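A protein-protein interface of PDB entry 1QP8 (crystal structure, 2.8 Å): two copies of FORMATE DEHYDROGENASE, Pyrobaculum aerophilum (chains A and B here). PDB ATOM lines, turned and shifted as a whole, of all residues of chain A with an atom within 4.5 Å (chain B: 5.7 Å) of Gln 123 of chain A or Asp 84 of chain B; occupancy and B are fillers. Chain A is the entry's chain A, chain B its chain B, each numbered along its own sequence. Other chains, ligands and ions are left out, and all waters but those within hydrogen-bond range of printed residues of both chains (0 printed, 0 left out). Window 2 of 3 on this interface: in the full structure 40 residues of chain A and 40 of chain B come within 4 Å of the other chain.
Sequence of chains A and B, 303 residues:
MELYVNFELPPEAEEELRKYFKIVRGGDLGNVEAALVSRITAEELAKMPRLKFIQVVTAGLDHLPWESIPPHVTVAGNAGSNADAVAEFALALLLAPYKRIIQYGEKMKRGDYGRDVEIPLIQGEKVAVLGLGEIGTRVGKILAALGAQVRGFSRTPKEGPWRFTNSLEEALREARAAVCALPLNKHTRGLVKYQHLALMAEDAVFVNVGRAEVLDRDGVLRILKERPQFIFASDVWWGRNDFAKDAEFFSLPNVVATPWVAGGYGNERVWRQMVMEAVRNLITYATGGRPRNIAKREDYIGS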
ATOM      1  N   LEU A 121      21.497  -8.591  -5.187  1.00  0.00           N
ATOM      2  CA  LEU A 121      20.462  -9.600  -5.221  1.00  0.00           C
ATOM      3  C   LEU A 121      19.540  -9.219  -6.363  1.00  0.00           C
ATOM      4  O   LEU A 121      19.458  -8.060  -6.748  1.00  0.00           O
ATOM      5  CB  LEU A 121      19.714  -9.647  -3.889  1.00  0.00           C
ATOM      6  CG  LEU A 121      19.973 -10.923  -3.071  1.00  0.00           C
ATOM      7  CD1 LEU A 121      21.462 -11.224  -3.020  1.00  0.00           C
ATOM      8  CD2 LEU A 121      19.431 -10.754  -1.670  1.00  0.00           C
ATOM      9  N   ILE A 122      18.882 -10.207  -6.941  1.00  0.00           N
ATOM     10  CA  ILE A 122      17.962  -9.944  -8.025  1.00  0.00           C
ATOM     11  C   ILE A 122      16.596  -9.723  -7.382  1.00  0.00           C
ATOM     12  O   ILE A 122      15.847  -8.802  -7.751  1.00  0.00           O
ATOM     13  CB  ILE A 122      17.966 -11.132  -9.021  1.00  0.00           C
ATOM     14  CG1 ILE A 122      19.120 -10.927 -10.008  1.00  0.00           C
ATOM     15  CG2 ILE A 122      16.618 -11.264  -9.737  1.00  0.00           C
ATOM     16  CD1 ILE A 122      19.245 -11.989 -11.042  1.00  0.00           C
ATOM     17  N   GLN A 123      16.308 -10.558  -6.390  1.00  0.00           N
ATOM     18  CA  GLN A 123      15.064 -10.488  -5.640  1.00  0.00           C
ATOM     19  C   GLN A 123      14.777  -9.045  -5.211  1.00  0.00           C
ATOM     20  O   GLN A 123      15.655  -8.351  -4.691  1.00  0.00           O
ATOM     21  CB  GLN A 123      15.171 -11.369  -4.402  1.00  0.00           C
ATOM     22  CG  GLN A 123      13.942 -12.184  -4.107  1.00  0.00           C
ATOM     23  CD  GLN A 123      13.578 -12.145  -2.644  1.00  0.00           C
ATOM     24  OE1 GLN A 123      13.026 -11.156  -2.163  1.00  0.00           O
ATOM     25  NE2 GLN A 123      13.901 -13.214  -1.921  1.00  0.00           N
ATOM     26  N   GLY A 124      13.548  -8.599  -5.435  1.00  0.00           N
ATOM     27  CA  GLY A 124      13.163  -7.252  -5.063  1.00  0.00           C
ATOM     28  C   GLY A 124      13.902  -6.145  -5.792  1.00  0.00           C
ATOM     29  O   GLY A 124      13.907  -4.997  -5.346  1.00  0.00           O
ATOM     30  N   GLU A 125      14.523  -6.459  -6.920  1.00  0.00           N
ATOM     31  CA  GLU A 125      15.254  -5.426  -7.635  1.00  0.00           C
ATOM     32  C   GLU A 125      14.531  -4.888  -8.861  1.00  0.00           C
ATOM     33  O   GLU A 125      13.791  -5.608  -9.530  1.00  0.00           O
ATOM     34  CB  GLU A 125      16.634  -5.942  -8.030  1.00  0.00           C
ATOM     35  N   LEU A 146      12.368 -14.777 -10.447  1.00  0.00           N
ATOM     36  CA  LEU A 146      13.512 -14.760  -9.543  1.00  0.00           C
ATOM     37  C   LEU A 146      13.277 -13.714  -8.461  1.00  0.00           C
ATOM     38  O   LEU A 146      14.125 -13.487  -7.587  1.00  0.00           O
ATOM     39  CB  LEU A 146      14.797 -14.435 -10.309  1.00  0.00           C
ATOM     40  CG  LEU A 146      15.393 -15.504 -11.226  1.00  0.00           C
ATOM     41  CD1 LEU A 146      16.640 -14.938 -11.870  1.00  0.00           C
ATOM     42  CD2 LEU A 146      15.727 -16.767 -10.440  1.00  0.00           C
ATOM     43  N   GLY A 147      12.119 -13.068  -8.539  1.00  0.00           N
ATOM     44  CA  GLY A 147      11.763 -12.064  -7.555  1.00  0.00           C
ATOM     45  C   GLY A 147      12.096 -10.643  -7.941  1.00  0.00           C
ATOM     46  O   GLY A 147      12.152  -9.768  -7.086  1.00  0.00           O
ATOM     47  N   GLY B  80      17.274 -21.825   4.177  1.00  0.00           N
ATOM     48  CA  GLY B  80      16.174 -21.176   3.491  1.00  0.00           C
ATOM     49  C   GLY B  80      16.215 -19.727   3.906  1.00  0.00           C
ATOM     50  O   GLY B  80      15.505 -18.875   3.374  1.00  0.00           O
ATOM     51  N   ASN B  82      18.721 -18.069   3.485  1.00  0.00           N
ATOM     52  CA  ASN B  82      19.510 -17.504   2.400  1.00  0.00           C
ATOM     53  C   ASN B  82      19.266 -18.279   1.108  1.00  0.00           C
ATOM     54  O   ASN B  82      20.031 -18.161   0.153  1.00  0.00           O
ATOM     55  CB  ASN B  82      20.986 -17.609   2.772  1.00  0.00           C
ATOM     56  CG  ASN B  82      21.393 -19.035   3.143  1.00  0.00           C
ATOM     57  OD1 ASN B  82      22.547 -19.293   3.489  1.00  0.00           O
ATOM     58  ND2 ASN B  82      20.444 -19.965   3.071  1.00  0.00           N
ATOM     59  N   ALA B  83      18.201 -19.072   1.089  1.00  0.00           N
ATOM     60  CA  ALA B  83      17.870 -19.900  -0.065  1.00  0.00           C
ATOM     61  C   ALA B  83      17.846 -19.128  -1.376  1.00  0.00           C
ATOM     62  O   ALA B  83      18.461 -19.537  -2.354  1.00  0.00           O
ATOM     63  CB  ALA B  83      16.536 -20.584   0.161  1.00  0.00           C
ATOM     64  N   ASP B  84      17.128 -18.016  -1.397  1.00  0.00           N
ATOM     65  CA  ASP B  84      17.037 -17.202  -2.594  1.00  0.00           C
ATOM     66  C   ASP B  84      18.403 -16.727  -3.064  1.00  0.00           C
ATOM     67  O   ASP B  84      18.803 -16.993  -4.195  1.00  0.00           O
ATOM     68  CB  ASP B  84      16.144 -15.988  -2.335  1.00  0.00           C
ATOM     69  CG  ASP B  84      14.670 -16.317  -2.427  1.00  0.00           C
ATOM     70  OD1 ASP B  84      14.265 -17.374  -1.904  1.00  0.00           O
ATOM     71  OD2 ASP B  84      13.912 -15.516  -3.016  1.00  0.00           O
ATOM     72  N   ALA B  85      19.115 -16.016  -2.193  1.00  0.00           N
ATOM     73  CA  ALA B  85      20.433 -15.482  -2.532  1.00  0.00           C
ATOM     74  C   ALA B  85      21.367 -16.543  -3.119  1.00  0.00           C
ATOM     75  O   ALA B  85      21.898 -16.380  -4.218  1.00  0.00           O
ATOM     76  CB  ALA B  85      21.069 -14.838  -1.301  1.00  0.00           C
ATOM     77  N   VAL B  86      21.571 -17.622  -2.382  1.00  0.00           N
ATOM     78  CA  VAL B  86      22.427 -18.688  -2.848  1.00  0.00           C
ATOM     79  C   VAL B  86      21.884 -19.282  -4.128  1.00  0.00           C
ATOM     80  O   VAL B  86      22.642 -19.728  -4.988  1.00  0.00           O
ATOM     81  CB  VAL B  86      22.518 -19.781  -1.820  1.00  0.00           C
ATOM     82  CG1 VAL B  86      23.260 -20.985  -2.386  1.00  0.00           C
ATOM     83  CG2 VAL B  86      23.202 -19.241  -0.599  1.00  0.00           C
ATOM     84  N   ALA B  87      20.564 -19.289  -4.257  1.00  0.00           N
ATOM     85  CA  ALA B  87      19.921 -19.842  -5.443  1.00  0.00           C
ATOM     86  C   ALA B  87      20.388 -19.110  -6.684  1.00  0.00           C
ATOM     87  O   ALA B  87      20.990 -19.709  -7.573  1.00  0.00           O
ATOM     88  CB  ALA B  87      18.408 -19.741  -5.316  1.00  0.00           C
ATOM     89  N   GLU B  88      20.115 -17.812  -6.742  1.00  0.00           N
ATOM     90  CA  GLU B  88      20.519 -17.042  -7.895  1.00  0.00           C
ATOM     91  C   GLU B  88      22.032 -17.077  -8.121  1.00  0.00           C
ATOM     92  O   GLU B  88      22.496 -17.005  -9.259  1.00  0.00           O
ATOM     93  CB  GLU B  88      19.993 -15.606  -7.794  1.00  0.00           C
ATOM     94  CG  GLU B  88      19.872 -15.031  -6.401  1.00  0.00           C
ATOM     95  CD  GLU B  88      19.214 -13.652  -6.406  1.00  0.00           C
ATOM     96  OE1 GLU B  88      17.963 -13.570  -6.464  1.00  0.00           O
ATOM     97  OE2 GLU B  88      19.954 -12.642  -6.369  1.00  0.00           O
ATOM     98  N   PHE B  89      22.807 -17.223  -7.054  1.00  0.00           N
ATOM     99  CA  PHE B  89      24.253 -17.283  -7.213  1.00  0.00           C
ATOM    100  C   PHE B  89      24.645 -18.561  -7.950  1.00  0.00           C
ATOM    101  O   PHE B  89      25.552 -18.547  -8.764  1.00  0.00           O
ATOM    102  CB  PHE B  89      24.958 -17.252  -5.854  1.00  0.00           C
ATOM    103  CG  PHE B  89      26.412 -16.891  -5.934  1.00  0.00           C
ATOM    104  CD1 PHE B  89      26.809 -15.560  -5.977  1.00  0.00           C
ATOM    105  CD2 PHE B  89      27.391 -17.890  -5.985  1.00  0.00           C
ATOM    106  CE1 PHE B  89      28.156 -15.225  -6.069  1.00  0.00           C
ATOM    107  CE2 PHE B  89      28.750 -17.569  -6.074  1.00  0.00           C
ATOM    108  CZ  PHE B  89      29.132 -16.236  -6.116  1.00  0.00           C
ATOM    109  N   GLU B 134      14.763 -25.998  -0.673  1.00  0.00           N
ATOM    110  CA  GLU B 134      15.320 -24.706  -0.272  1.00  0.00           C
ATOM    111  C   GLU B 134      16.149 -24.124  -1.396  1.00  0.00           C
ATOM    112  O   GLU B 134      15.664 -23.289  -2.163  1.00  0.00           O
ATOM    113  CB  GLU B 134      16.175 -24.863   0.978  1.00  0.00           C
ATOM    114  CG  GLU B 134      15.604 -25.843   1.977  1.00  0.00           C
ATOM    115  CD  GLU B 134      16.619 -26.238   3.016  1.00  0.00           C
ATOM    116  OE1 GLU B 134      16.774 -25.479   3.996  1.00  0.00           O
ATOM    117  OE2 GLU B 134      17.273 -27.293   2.841  1.00  0.00           O
ATOM    118  N   ARG B 138      14.847 -24.391  -5.572  1.00  0.00           N
ATOM    119  CA  ARG B 138      14.695 -23.156  -6.329  1.00  0.00           C
ATOM    120  C   ARG B 138      15.485 -23.258  -7.618  1.00  0.00           C
ATOM    121  O   ARG B 138      15.024 -22.828  -8.677  1.00  0.00           O
ATOM    122  CB  ARG B 138      15.181 -21.953  -5.530  1.00  0.00           C
ATOM    123  CG  ARG B 138      14.146 -21.362  -4.600  1.00  0.00           C
ATOM    124  CD  ARG B 138      14.610 -20.007  -4.100  1.00  0.00           C
ATOM    125  NE  ARG B 138      13.781 -19.475  -3.023  1.00  0.00           N
ATOM    126  CZ  ARG B 138      13.589 -20.071  -1.847  1.00  0.00           C
ATOM    127  NH1 ARG B 138      14.165 -21.243  -1.576  1.00  0.00           N
ATOM    128  NH2 ARG B 138      12.825 -19.480  -0.931  1.00  0.00           N
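NE2 of Gln 123 of chain A is in hydrogen-bond range of OD2 of Asp 84 of chain B (2.5 Å).
The backbone NH of Gln 123 of chain A lies within hydrogen-bond range of the side-chain carboxylate of Glu 88 of chain B (3.4 Å).
The backbone NH (N) of Ile 122 of chain A is in hydrogen-bond range of the side-chain carboxylate (OE2) of Glu 88 of chain B.
The side-chain carboxylate of Asp 84 of chain B is in salt-bridge range of the guanidinium group of Arg 138 of chain B.
Among the printed residues, merely in contact across the chains: Leu 121 of chain A with Glu 88 of chain B (3.3 Å) and Leu 146 of chain A with Glu 88 of chain B (3.9998 Å).
Printed residues of chain B within 4 Å of Leu 121 of chain A: Glu 88.
Printed residues of chain B within 4 Å of Gln 123 of chain A: Asp 84 and Glu 88.
Gly 147 of chain A touches none of the printed residues of chain B.
Gly 80 of chain B touches none of the printed residues of chain A.
Of the printed residues of chain A, Asp 84 of chain B touches Gln 123 (2.5 Å).
Of the printed residues of chain A, Glu 88 of chain B touches Leu 121 (3.3 Å), Ile 122 (2.7 Å), Gln 123 (3.4 Å) and Leu 146 (3.9998 Å).
The nearest printed residue of chain B that does not touch Gln 123 of chain A is Ala 85 of chain B (5.9 Å).
Of the 7 printed residues of chain A, 4 touch a printed residue of chain B.
Printed residues of chain A that touch a printed residue of chain B: Leu 121, Ile 122, Gln 123 and Leu 146.
Along chain A the printed residues that touch a printed residue of chain B span positions 121 to 146.
Of the 11 printed residues of chain B, 2 touch a printed residue of chain A.
Among the printed residues, no Asp or Glu carboxylate lies within 4 Å of a Lys or Arg side-chain nitrogen of the other chain.
No position is printed for both chains.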
